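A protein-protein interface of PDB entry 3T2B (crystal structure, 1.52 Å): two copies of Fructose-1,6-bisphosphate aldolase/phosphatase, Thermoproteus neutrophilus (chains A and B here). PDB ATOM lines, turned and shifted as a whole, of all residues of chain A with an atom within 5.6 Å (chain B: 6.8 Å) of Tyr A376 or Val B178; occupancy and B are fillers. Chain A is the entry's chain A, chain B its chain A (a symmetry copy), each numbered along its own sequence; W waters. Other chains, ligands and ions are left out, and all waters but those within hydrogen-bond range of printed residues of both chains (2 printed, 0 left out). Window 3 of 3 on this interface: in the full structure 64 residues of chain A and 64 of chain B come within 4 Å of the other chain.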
ATOM      1  N   LYS A 369     -23.125  31.746  -2.878  1.00  0.00           N
ATOM      2  CA  LYS A 369     -24.237  31.147  -3.576  1.00  0.00           C
ATOM      3  C   LYS A 369     -23.915  29.787  -4.122  1.00  0.00           C
ATOM      4  O   LYS A 369     -22.904  29.634  -4.825  1.00  0.00           O
ATOM      5  CB  LYS A 369     -24.655  32.047  -4.744  1.00  0.00           C
ATOM      6  CG  LYS A 369     -25.961  31.560  -5.471  1.00  0.00           C
ATOM      7  CD  LYS A 369     -26.072  32.259  -6.861  1.00  0.00           C
ATOM      8  CE  LYS A 369     -27.520  32.435  -7.383  1.00  0.00           C
ATOM      9  NZ  LYS A 369     -28.553  31.510  -6.785  1.00  0.00           N
ATOM     10  N   PRO A 370     -24.758  28.776  -3.832  1.00  0.00           N
ATOM     11  CA  PRO A 370     -24.601  27.456  -4.462  1.00  0.00           C
ATOM     12  C   PRO A 370     -25.328  27.291  -5.769  1.00  0.00           C
ATOM     13  O   PRO A 370     -26.399  27.928  -6.008  1.00  0.00           O
ATOM     14  CB  PRO A 370     -25.231  26.505  -3.441  1.00  0.00           C
ATOM     15  CG  PRO A 370     -26.405  27.350  -2.916  1.00  0.00           C
ATOM     16  CD  PRO A 370     -25.803  28.743  -2.771  1.00  0.00           C
ATOM     17  N   TYR A 371     -24.796  26.450  -6.613  1.00  0.00           N
ATOM     18  CA  TYR A 371     -25.499  26.090  -7.819  1.00  0.00           C
ATOM     19  C   TYR A 371     -25.667  24.611  -7.785  1.00  0.00           C
ATOM     20  O   TYR A 371     -24.695  23.855  -7.723  1.00  0.00           O
ATOM     21  CB  TYR A 371     -24.685  26.462  -9.057  1.00  0.00           C
ATOM     22  CG  TYR A 371     -24.416  27.929  -9.128  1.00  0.00           C
ATOM     23  CD1 TYR A 371     -25.398  28.825  -9.631  1.00  0.00           C
ATOM     24  CD2 TYR A 371     -23.208  28.482  -8.714  1.00  0.00           C
ATOM     25  CE1 TYR A 371     -25.137  30.206  -9.701  1.00  0.00           C
ATOM     26  CE2 TYR A 371     -22.957  29.835  -8.761  1.00  0.00           C
ATOM     27  CZ  TYR A 371     -23.927  30.711  -9.273  1.00  0.00           C
ATOM     28  OH  TYR A 371     -23.661  32.054  -9.311  1.00  0.00           O
ATOM     29  N   PRO A 372     -26.925  24.094  -7.852  1.00  0.00           N
ATOM     30  CA  PRO A 372     -27.032  22.636  -8.133  1.00  0.00           C
ATOM     31  C   PRO A 372     -26.158  22.217  -9.281  1.00  0.00           C
ATOM     32  O   PRO A 372     -26.178  22.879 -10.366  1.00  0.00           O
ATOM     33  CB  PRO A 372     -28.552  22.408  -8.476  1.00  0.00           C
ATOM     34  CG  PRO A 372     -29.197  23.642  -7.808  1.00  0.00           C
ATOM     35  CD  PRO A 372     -28.230  24.808  -7.790  1.00  0.00           C
ATOM     36  N   ALA A 373     -25.338  21.182  -9.046  1.00  0.00           N
ATOM     37  CA  ALA A 373     -24.295  20.809 -10.011  1.00  0.00           C
ATOM     38  C   ALA A 373     -24.771  20.367 -11.390  1.00  0.00           C
ATOM     39  O   ALA A 373     -24.083  20.632 -12.364  1.00  0.00           O
ATOM     40  CB  ALA A 373     -23.283  19.760  -9.430  1.00  0.00           C
ATOM     41  N   ASP A 374     -25.923  19.700 -11.494  1.00  0.00           N
ATOM     42  CA  ASP A 374     -26.433  19.341 -12.865  1.00  0.00           C
ATOM     43  C   ASP A 374     -26.781  20.559 -13.744  1.00  0.00           C
ATOM     44  O   ASP A 374     -26.256  20.742 -14.870  1.00  0.00           O
ATOM     45  CB  ASP A 374     -27.605  18.401 -12.777  1.00  0.00           C
ATOM     46  CG  ASP A 374     -27.235  17.067 -12.195  1.00  0.00           C
ATOM     47  OD1 ASP A 374     -26.134  16.558 -12.500  1.00  0.00           O
ATOM     48  OD2 ASP A 374     -28.052  16.519 -11.422  1.00  0.00           O
ATOM     49  N   GLN A 375     -27.552  21.468 -13.195  1.00  0.00           N
ATOM     50  CA  GLN A 375     -27.865  22.676 -13.966  1.00  0.00           C
ATOM     51  C   GLN A 375     -26.661  23.549 -14.207  1.00  0.00           C
ATOM     52  O   GLN A 375     -26.601  24.279 -15.192  1.00  0.00           O
ATOM     53  CB  GLN A 375     -29.000  23.544 -13.348  1.00  0.00           C
ATOM     54  CG  GLN A 375     -28.923  23.842 -11.836  1.00  0.00           C
ATOM     55  CD  GLN A 375     -30.275  24.390 -11.216  1.00  0.00           C
ATOM     56  OE1 GLN A 375     -30.372  25.581 -10.851  1.00  0.00           O
ATOM     57  NE2 GLN A 375     -31.288  23.495 -11.063  1.00  0.00           N
ATOM     58  N   TYR A 376     -25.719  23.528 -13.261  1.00  0.00           N
ATOM     59  CA  TYR A 376     -24.543  24.368 -13.404  1.00  0.00           C
ATOM     60  C   TYR A 376     -23.787  24.068 -14.688  1.00  0.00           C
ATOM     61  O   TYR A 376     -23.375  25.021 -15.321  1.00  0.00           O
ATOM     62  CB  TYR A 376     -23.605  24.260 -12.185  1.00  0.00           C
ATOM     63  CG  TYR A 376     -22.302  25.054 -12.365  1.00  0.00           C
ATOM     64  CD1 TYR A 376     -21.169  24.429 -12.954  1.00  0.00           C
ATOM     65  CD2 TYR A 376     -22.203  26.380 -11.955  1.00  0.00           C
ATOM     66  CE1 TYR A 376     -19.972  25.180 -13.163  1.00  0.00           C
ATOM     67  CE2 TYR A 376     -21.013  27.126 -12.195  1.00  0.00           C
ATOM     68  CZ  TYR A 376     -19.911  26.465 -12.743  1.00  0.00           C
ATOM     69  OH  TYR A 376     -18.777  27.204 -12.909  1.00  0.00           O
ATOM     70  N   GLU A 377     -23.588  22.791 -15.037  1.00  0.00           N
ATOM     71  CA  GLU A 377     -22.973  22.373 -16.323  1.00  0.00           C
ATOM     72  C   GLU A 377     -23.422  23.153 -17.585  1.00  0.00           C
ATOM     73  O   GLU A 377     -22.568  23.640 -18.370  1.00  0.00           O
ATOM     74  CB  GLU A 377     -23.251  20.889 -16.584  1.00  0.00           C
ATOM     75  CG  GLU A 377     -22.461  19.935 -15.728  1.00  0.00           C
ATOM     76  CD  GLU A 377     -20.928  20.169 -15.870  1.00  0.00           C
ATOM     77  OE1 GLU A 377     -20.516  21.011 -16.711  1.00  0.00           O
ATOM     78  OE2 GLU A 377     -20.155  19.483 -15.169  1.00  0.00           O
ATOM     79  N   LYS A 378     -24.742  23.257 -17.801  1.00  0.00           N
ATOM     80  CA  LYS A 378     -25.284  24.071 -18.954  1.00  0.00           C
ATOM     81  C   LYS A 378     -24.958  25.569 -18.861  1.00  0.00           C
ATOM     82  O   LYS A 378     -24.780  26.240 -19.886  1.00  0.00           O
ATOM     83  CB  LYS A 378     -26.826  23.947 -19.063  1.00  0.00           C
ATOM     84  CG  LYS A 378     -27.419  22.529 -18.776  1.00  0.00           C
ATOM     85  CD  LYS A 378     -28.961  22.442 -18.978  1.00  0.00           C
ATOM     86  CE  LYS A 378     -29.726  23.546 -18.190  1.00  0.00           C
ATOM     87  NZ  LYS A 378     -29.685  23.433 -16.695  1.00  0.00           N
ATOM     88  N   ASP A 379     -24.932  26.106 -17.656  1.00  0.00           N
ATOM     89  CA  ASP A 379     -24.853  27.564 -17.445  1.00  0.00           C
ATOM     90  C   ASP A 379     -23.443  28.100 -17.084  1.00  0.00           C
ATOM     91  O   ASP A 379     -23.279  29.315 -16.829  1.00  0.00           O
ATOM     92  CB  ASP A 379     -25.774  27.980 -16.317  1.00  0.00           C
ATOM     93  CG  ASP A 379     -27.261  27.778 -16.644  1.00  0.00           C
ATOM     94  OD1 ASP A 379     -27.635  27.861 -17.867  1.00  0.00           O
ATOM     95  OD2 ASP A 379     -28.000  27.513 -15.655  1.00  0.00           O
ATOM     96  N   ARG A 380     -22.455  27.188 -17.027  1.00  0.00           N
ATOM     97  CA  ARG A 380     -21.089  27.561 -16.545  1.00  0.00           C
ATOM     98  C   ARG A 380     -20.575  28.816 -17.292  1.00  0.00           C
ATOM     99  O   ARG A 380     -20.190  29.815 -16.700  1.00  0.00           O
ATOM    100  CB  ARG A 380     -20.097  26.394 -16.718  1.00  0.00           C
ATOM    101  CG  ARG A 380     -18.595  26.874 -16.442  1.00  0.00           C
ATOM    102  CD  ARG A 380     -17.542  25.794 -16.726  1.00  0.00           C
ATOM    103  NE  ARG A 380     -17.675  24.722 -15.753  1.00  0.00           N
ATOM    104  CZ  ARG A 380     -17.751  23.429 -16.019  1.00  0.00           C
ATOM    105  NH1 ARG A 380     -17.722  22.962 -17.292  1.00  0.00           N
ATOM    106  NH2 ARG A 380     -17.903  22.573 -15.024  1.00  0.00           N
ATOM    107  N   TYR A 383     -22.321  31.873 -16.182  1.00  0.00           N
ATOM    108  CA  TYR A 383     -22.010  32.266 -14.799  1.00  0.00           C
ATOM    109  C   TYR A 383     -20.636  32.848 -14.726  1.00  0.00           C
ATOM    110  O   TYR A 383     -20.418  33.790 -13.991  1.00  0.00           O
ATOM    111  CB  TYR A 383     -22.108  31.093 -13.840  1.00  0.00           C
ATOM    112  CG  TYR A 383     -23.496  30.558 -13.623  1.00  0.00           C
ATOM    113  CD1 TYR A 383     -24.594  31.422 -13.381  1.00  0.00           C
ATOM    114  CD2 TYR A 383     -23.722  29.195 -13.626  1.00  0.00           C
ATOM    115  CE1 TYR A 383     -25.873  30.903 -13.170  1.00  0.00           C
ATOM    116  CE2 TYR A 383     -24.978  28.663 -13.418  1.00  0.00           C
ATOM    117  CZ  TYR A 383     -26.056  29.515 -13.202  1.00  0.00           C
ATOM    118  OH  TYR A 383     -27.283  28.928 -12.995  1.00  0.00           O
ATOM    119  N   ILE A 384     -19.700  32.308 -15.510  1.00  0.00           N
ATOM    120  CA  ILE A 384     -18.324  32.873 -15.531  1.00  0.00           C
ATOM    121  C   ILE A 384     -18.292  34.220 -16.231  1.00  0.00           C
ATOM    122  O   ILE A 384     -17.656  35.188 -15.738  1.00  0.00           O
ATOM    123  CB  ILE A 384     -17.311  31.925 -16.224  1.00  0.00           C
ATOM    124  CG1 ILE A 384     -17.215  30.541 -15.537  1.00  0.00           C
ATOM    125  CG2 ILE A 384     -15.981  32.642 -16.350  1.00  0.00           C
ATOM    126  CD1 ILE A 384     -16.764  30.527 -14.086  1.00  0.00           C
ATOM    127  N   ILE B 167     -10.898  32.943 -10.540  1.00  0.00           N
ATOM    128  CA  ILE B 167     -12.222  32.359 -10.172  1.00  0.00           C
ATOM    129  C   ILE B 167     -12.039  30.859  -9.982  1.00  0.00           C
ATOM    130  O   ILE B 167     -11.574  30.134 -10.860  1.00  0.00           O
ATOM    131  CB  ILE B 167     -13.269  32.604 -11.335  1.00  0.00           C
ATOM    132  CG1 ILE B 167     -13.336  34.087 -11.595  1.00  0.00           C
ATOM    133  CG2 ILE B 167     -14.630  32.114 -10.814  1.00  0.00           C
ATOM    134  CD1 ILE B 167     -13.999  34.373 -13.015  1.00  0.00           C
ATOM    135  N   PHE B 168     -12.423  30.386  -8.779  1.00  0.00           N
ATOM    136  CA  PHE B 168     -12.326  28.943  -8.491  1.00  0.00           C
ATOM    137  C   PHE B 168     -13.731  28.328  -8.533  1.00  0.00           C
ATOM    138  O   PHE B 168     -14.653  28.881  -7.846  1.00  0.00           O
ATOM    139  CB  PHE B 168     -11.826  28.762  -7.031  1.00  0.00           C
ATOM    140  CG  PHE B 168     -10.345  29.149  -6.846  1.00  0.00           C
ATOM    141  CD1 PHE B 168      -9.935  30.512  -6.744  1.00  0.00           C
ATOM    142  CD2 PHE B 168      -9.423  28.107  -6.718  1.00  0.00           C
ATOM    143  CE1 PHE B 168      -8.507  30.815  -6.611  1.00  0.00           C
ATOM    144  CE2 PHE B 168      -8.017  28.461  -6.565  1.00  0.00           C
ATOM    145  CZ  PHE B 168      -7.618  29.777  -6.515  1.00  0.00           C
ATOM    146  N   GLU B 169     -13.869  27.305  -9.322  1.00  0.00           N
ATOM    147  CA  GLU B 169     -15.100  26.488  -9.318  1.00  0.00           C
ATOM    148  C   GLU B 169     -14.851  25.320  -8.385  1.00  0.00           C
ATOM    149  O   GLU B 169     -14.057  24.430  -8.724  1.00  0.00           O
ATOM    150  CB  GLU B 169     -15.348  26.043 -10.764  1.00  0.00           C
ATOM    151  CG  GLU B 169     -16.623  25.158 -10.932  1.00  0.00           C
ATOM    152  CD  GLU B 169     -16.763  24.656 -12.338  1.00  0.00           C
ATOM    153  OE1 GLU B 169     -16.763  23.435 -12.549  1.00  0.00           O
ATOM    154  OE2 GLU B 169     -16.745  25.590 -13.232  1.00  0.00           O
ATOM    155  N   VAL B 170     -15.651  25.285  -7.327  1.00  0.00           N
ATOM    156  CA  VAL B 170     -15.478  24.326  -6.165  1.00  0.00           C
ATOM    157  C   VAL B 170     -16.668  23.368  -6.220  1.00  0.00           C
ATOM    158  O   VAL B 170     -17.808  23.888  -6.230  1.00  0.00           O
ATOM    159  CB  VAL B 170     -15.431  25.087  -4.867  1.00  0.00           C
ATOM    160  CG1 VAL B 170     -15.324  24.098  -3.638  1.00  0.00           C
ATOM    161  CG2 VAL B 170     -14.089  25.917  -4.859  1.00  0.00           C
ATOM    162  N   LEU B 171     -16.441  22.077  -6.278  1.00  0.00           N
ATOM    163  CA  LEU B 171     -17.507  21.095  -6.292  1.00  0.00           C
ATOM    164  C   LEU B 171     -17.635  20.474  -4.885  1.00  0.00           C
ATOM    165  O   LEU B 171     -16.620  19.947  -4.345  1.00  0.00           O
ATOM    166  CB  LEU B 171     -17.220  20.008  -7.301  1.00  0.00           C
ATOM    167  CG  LEU B 171     -18.227  18.814  -7.395  1.00  0.00           C
ATOM    168  CD1 LEU B 171     -19.676  19.446  -7.747  1.00  0.00           C
ATOM    169  CD2 LEU B 171     -17.769  17.800  -8.379  1.00  0.00           C
ATOM    170  N   ASP B 172     -18.796  20.564  -4.256  1.00  0.00           N
ATOM    171  CA  ASP B 172     -19.149  19.769  -3.070  1.00  0.00           C
ATOM    172  C   ASP B 172     -19.520  18.435  -3.575  1.00  0.00           C
ATOM    173  O   ASP B 172     -20.594  18.227  -4.222  1.00  0.00           O
ATOM    174  CB  ASP B 172     -20.313  20.474  -2.335  1.00  0.00           C
ATOM    175  CG  ASP B 172     -20.893  19.633  -1.170  1.00  0.00           C
ATOM    176  OD1 ASP B 172     -20.546  18.462  -1.045  1.00  0.00           O
ATOM    177  OD2 ASP B 172     -21.707  20.279  -0.490  1.00  0.00           O
ATOM    178  N   HIS B 176     -23.377  17.553  -4.095  1.00  0.00           N
ATOM    179  CA  HIS B 176     -23.464  17.854  -5.539  1.00  0.00           C
ATOM    180  C   HIS B 176     -23.852  19.326  -5.806  1.00  0.00           C
ATOM    181  O   HIS B 176     -24.900  19.657  -6.464  1.00  0.00           O
ATOM    182  CB  HIS B 176     -24.317  16.805  -6.297  1.00  0.00           C
ATOM    183  CG  HIS B 176     -23.934  16.626  -7.740  1.00  0.00           C
ATOM    184  ND1 HIS B 176     -22.615  16.622  -8.198  1.00  0.00           N
ATOM    185  CD2 HIS B 176     -24.710  16.401  -8.846  1.00  0.00           C
ATOM    186  CE1 HIS B 176     -22.604  16.441  -9.512  1.00  0.00           C
ATOM    187  NE2 HIS B 176     -23.861  16.305  -9.928  1.00  0.00           N
ATOM    188  N   LYS B 177     -23.068  20.276  -5.269  1.00  0.00           N
ATOM    189  CA  LYS B 177     -23.371  21.706  -5.348  1.00  0.00           C
ATOM    190  C   LYS B 177     -22.064  22.353  -5.832  1.00  0.00           C
ATOM    191  O   LYS B 177     -21.007  21.892  -5.377  1.00  0.00           O
ATOM    192  CB  LYS B 177     -23.751  22.253  -4.035  1.00  0.00           C
ATOM    193  CG  LYS B 177     -25.131  21.659  -3.569  1.00  0.00           C
ATOM    194  CD  LYS B 177     -25.483  22.211  -2.272  1.00  0.00           C
ATOM    195  CE  LYS B 177     -26.843  21.596  -1.894  1.00  0.00           C
ATOM    196  NZ  LYS B 177     -27.162  21.932  -0.483  1.00  0.00           N
ATOM    197  N   VAL B 178     -22.134  23.351  -6.684  1.00  0.00           N
ATOM    198  CA  VAL B 178     -20.980  24.113  -7.171  1.00  0.00           C
ATOM    199  C   VAL B 178     -20.946  25.478  -6.556  1.00  0.00           C
ATOM    200  O   VAL B 178     -21.969  26.178  -6.389  1.00  0.00           O
ATOM    201  CB  VAL B 178     -20.987  24.236  -8.705  1.00  0.00           C
ATOM    202  CG1 VAL B 178     -19.912  25.158  -9.210  1.00  0.00           C
ATOM    203  CG2 VAL B 178     -20.953  22.918  -9.343  1.00  0.00           C
ATOM    204  N   TYR B 179     -19.756  25.958  -6.173  1.00  0.00           N
ATOM    205  CA  TYR B 179     -19.547  27.289  -5.682  1.00  0.00           C
ATOM    206  C   TYR B 179     -18.527  28.014  -6.550  1.00  0.00           C
ATOM    207  O   TYR B 179     -17.595  27.350  -6.993  1.00  0.00           O
ATOM    208  CB  TYR B 179     -19.055  27.281  -4.210  1.00  0.00           C
ATOM    209  CG  TYR B 179     -20.058  26.539  -3.285  1.00  0.00           C
ATOM    210  CD1 TYR B 179     -20.044  25.138  -3.168  1.00  0.00           C
ATOM    211  CD2 TYR B 179     -21.033  27.280  -2.601  1.00  0.00           C
ATOM    212  CE1 TYR B 179     -21.017  24.463  -2.367  1.00  0.00           C
ATOM    213  CE2 TYR B 179     -21.960  26.672  -1.821  1.00  0.00           C
ATOM    214  CZ  TYR B 179     -21.978  25.278  -1.701  1.00  0.00           C
ATOM    215  OH  TYR B 179     -22.942  24.706  -0.843  1.00  0.00           O
ATOM    216  N   LEU B 180     -18.711  29.308  -6.853  1.00  0.00           N
ATOM    217  CA  LEU B 180     -17.750  30.131  -7.542  1.00  0.00           C
ATOM    218  C   LEU B 180     -17.219  31.148  -6.613  1.00  0.00           C
ATOM    219  O   LEU B 180     -17.945  32.049  -6.060  1.00  0.00           O
ATOM    220  CB  LEU B 180     -18.404  30.871  -8.747  1.00  0.00           C
ATOM    221  CG  LEU B 180     -18.778  29.891  -9.769  1.00  0.00           C
ATOM    222  CD1 LEU B 180     -19.596  30.692 -10.960  1.00  0.00           C
ATOM    223  CD2 LEU B 180     -17.514  29.255 -10.458  1.00  0.00           C
ATOM    224  N   ARG B 203     -12.402  22.181  -8.987  1.00  0.00           N
ATOM    225  CA  ARG B 203     -12.576  21.419 -10.190  1.00  0.00           C
ATOM    226  C   ARG B 203     -11.992  22.191 -11.423  1.00  0.00           C
ATOM    227  O   ARG B 203     -11.384  21.570 -12.261  1.00  0.00           O
ATOM    228  CB  ARG B 203     -14.088  21.154 -10.415  1.00  0.00           C
ATOM    229  CG  ARG B 203     -14.289  20.231 -11.632  1.00  0.00           C
ATOM    230  CD  ARG B 203     -15.805  19.634 -11.740  1.00  0.00           C
ATOM    231  NE  ARG B 203     -16.739  20.768 -11.701  1.00  0.00           N
ATOM    232  CZ  ARG B 203     -18.085  20.626 -11.721  1.00  0.00           C
ATOM    233  NH1 ARG B 203     -18.590  19.396 -11.690  1.00  0.00           N
ATOM    234  NH2 ARG B 203     -18.877  21.726 -11.714  1.00  0.00           N
ATOM    235  N   LYS B 204     -12.253  23.500 -11.366  1.00  0.00           N
ATOM    236  CA  LYS B 204     -11.702  24.375 -12.452  1.00  0.00           C
ATOM    237  C   LYS B 204     -11.309  25.700 -11.890  1.00  0.00           C
ATOM    238  O   LYS B 204     -11.773  26.184 -10.863  1.00  0.00           O
ATOM    239  CB  LYS B 204     -12.818  24.649 -13.625  1.00  0.00           C
ATOM    240  CG  LYS B 204     -13.169  23.342 -14.354  1.00  0.00           C
ATOM    241  CD  LYS B 204     -14.169  23.342 -15.578  1.00  0.00           C
ATOM    242  CE  LYS B 204     -14.121  21.902 -16.282  1.00  0.00           C
ATOM    243  NZ  LYS B 204     -13.025  21.916 -17.451  1.00  0.00           N
ATOM    244  N   PHE B 206     -10.439  29.715 -13.489  1.00  0.00           N
ATOM    245  CA  PHE B 206     -10.486  30.681 -14.622  1.00  0.00           C
ATOM    246  C   PHE B 206      -9.827  31.937 -14.262  1.00  0.00           C
ATOM    247  O   PHE B 206      -9.897  32.436 -13.160  1.00  0.00           O
ATOM    248  CB  PHE B 206     -12.021  30.950 -14.940  1.00  0.00           C
ATOM    249  CG  PHE B 206     -12.753  29.752 -15.287  1.00  0.00           C
ATOM    250  CD1 PHE B 206     -12.725  29.179 -16.576  1.00  0.00           C
ATOM    251  CD2 PHE B 206     -13.480  29.082 -14.309  1.00  0.00           C
ATOM    252  CE1 PHE B 206     -13.448  27.979 -16.887  1.00  0.00           C
ATOM    253  CE2 PHE B 206     -14.152  27.885 -14.602  1.00  0.00           C
ATOM    254  CZ  PHE B 206     -14.141  27.326 -15.872  1.00  0.00           C
HETATM  255  O   HOH W   1     -21.296  20.574 -12.408  1.00  0.00           O
HETATM  256  O   HOH W   2     -21.033  30.817  -5.796  1.00  0.00           O
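Tyr A376 touches four residues of chain B.
Of chain A, only Lys A369 (3.9 Å), Pro A370 (3.5 Å), Tyr A371 (2.8 Å), Ala A373 (3.9 Å) and Tyr A376 (3.7 Å) come within 4 Å of Val B178.
Printed residues of chain A within 4 Å of Arg B203: Tyr A376 (3.8 Å), Glu A377 (3.8 Å) and Arg A380 (3.6 Å).
Of the printed residues of chain B, Glu A377 touches Arg B203 (3.8 Å).
Of the printed residues of chain A, Phe B206 touches Arg A380 (3.8 Å) and Ile A384 (3.6 Å).
Lys A378 touches none of the printed residues of chain B.
The nearest residue of chain B that does not touch Tyr A376 is Phe B206 (5.0 Å).
The nearest residue of chain A that does not touch Val B178 is Pro A372 (4.9 Å).
O of Val B170 is in hydrogen-bond range of N of Tyr B179.
The backbone NH of Ile B167 is in hydrogen-bond range of the backbone carbonyl oxygen of Phe B206 (2.9 Å).
The side-chain carboxylate (OE1) of Glu B169 lies within salt-bridge range of the guanidinium group (NE) of Arg B203, at 2.8 Å.
NH1 of Arg A380 lies within salt-bridge range of OE1 of Glu A377.
The backbone NH (N) of Asp B172 lies within hydrogen-bond range of the backbone carbonyl oxygen (O) of Lys B177, at 2.8 Å.
The side-chain carboxylate (OD2) of Asp A379 lies within hydrogen-bond range of the side-chain hydroxyl (OH) of Tyr A383.
Of the 14 printed residues of chain B, 10 touch a printed residue of chain A.
Hydrophobic or aromatic side chains of chain B within 4 Å of the printed part of chain A: Leu B171, His B176, Val B178, Tyr B179, Leu B180 and Phe B206.
Of the 14 printed residues of chain A, 10 touch a printed residue of chain B.
Among the printed residues, 22 pairs touch across the chains.
Water W2 lies within hydrogen-bond range of O of Lys A369 (2.4 Å) and N of Leu B180 (3.0 Å).
Water W1 lies within hydrogen-bond range of the guanidinium group (NH2) of Arg B203, the backbone carbonyl oxygen (O) of Ala A373 and the side-chain carboxylate (OE2) of Glu A377.
OD1 of Asp A374 is in hydrogen-bond range of NE2 of His B176, at 3.4 Å.
The backbone NH (N) of Ala A373 sits at hydrogen-bond distance from the backbone carbonyl oxygen (O) of His B176 (3.0 Å).
NH1 of Arg B203 is in salt-bridge range of OE2 of Glu A377, at 3.8 Å.
The backbone carbonyl oxygen of Tyr A371 is in hydrogen-bond range of the backbone NH of Val B178 (2.8 Å).
The side-chain hydroxyl (OH) of Tyr A376 lies within hydrogen-bond range of the side-chain carboxylate (OE2) of Glu B169 (2.6 Å).
The guanidinium group (NE) of Arg A380 lies within salt-bridge range of the side-chain carboxylate (OE2) of Glu B169, 2.8 Å away.
No position is printed for both chains.
Of the 22 pairs that touch across the chains among the printed residues, none has its exchanged pair printed and touching as well.
Among the printed residues, merely in contact across the chains: Tyr A376 with Leu B180 (3.4 Å), Tyr A371 with Lys B177 (3.5 Å), Pro A370 with Val B178 (3.5 Å), Arg A380 with Arg B203 (3.6 Å), Ile A384 with Phe B206 (3.6 Å), Arg A380 with Lys B204 (3.6 Å), Pro A370 with Tyr B179 (3.7 Å), Lys A369 with Tyr B179 (3.7 Å), Tyr A376 with Val B178 (3.7 Å), Tyr A376 with Arg B203 (3.8 Å), Arg A380 with Phe B206 (3.8 Å), Tyr A383 with Leu B180 (3.8 Å), Lys A369 with Val B178 (3.9 Å), Ile A384 with Leu B180 (3.9 Å), Ala A373 with Val B178 (3.9 Å) and Ala A373 with Leu B171 (3.99 Å).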
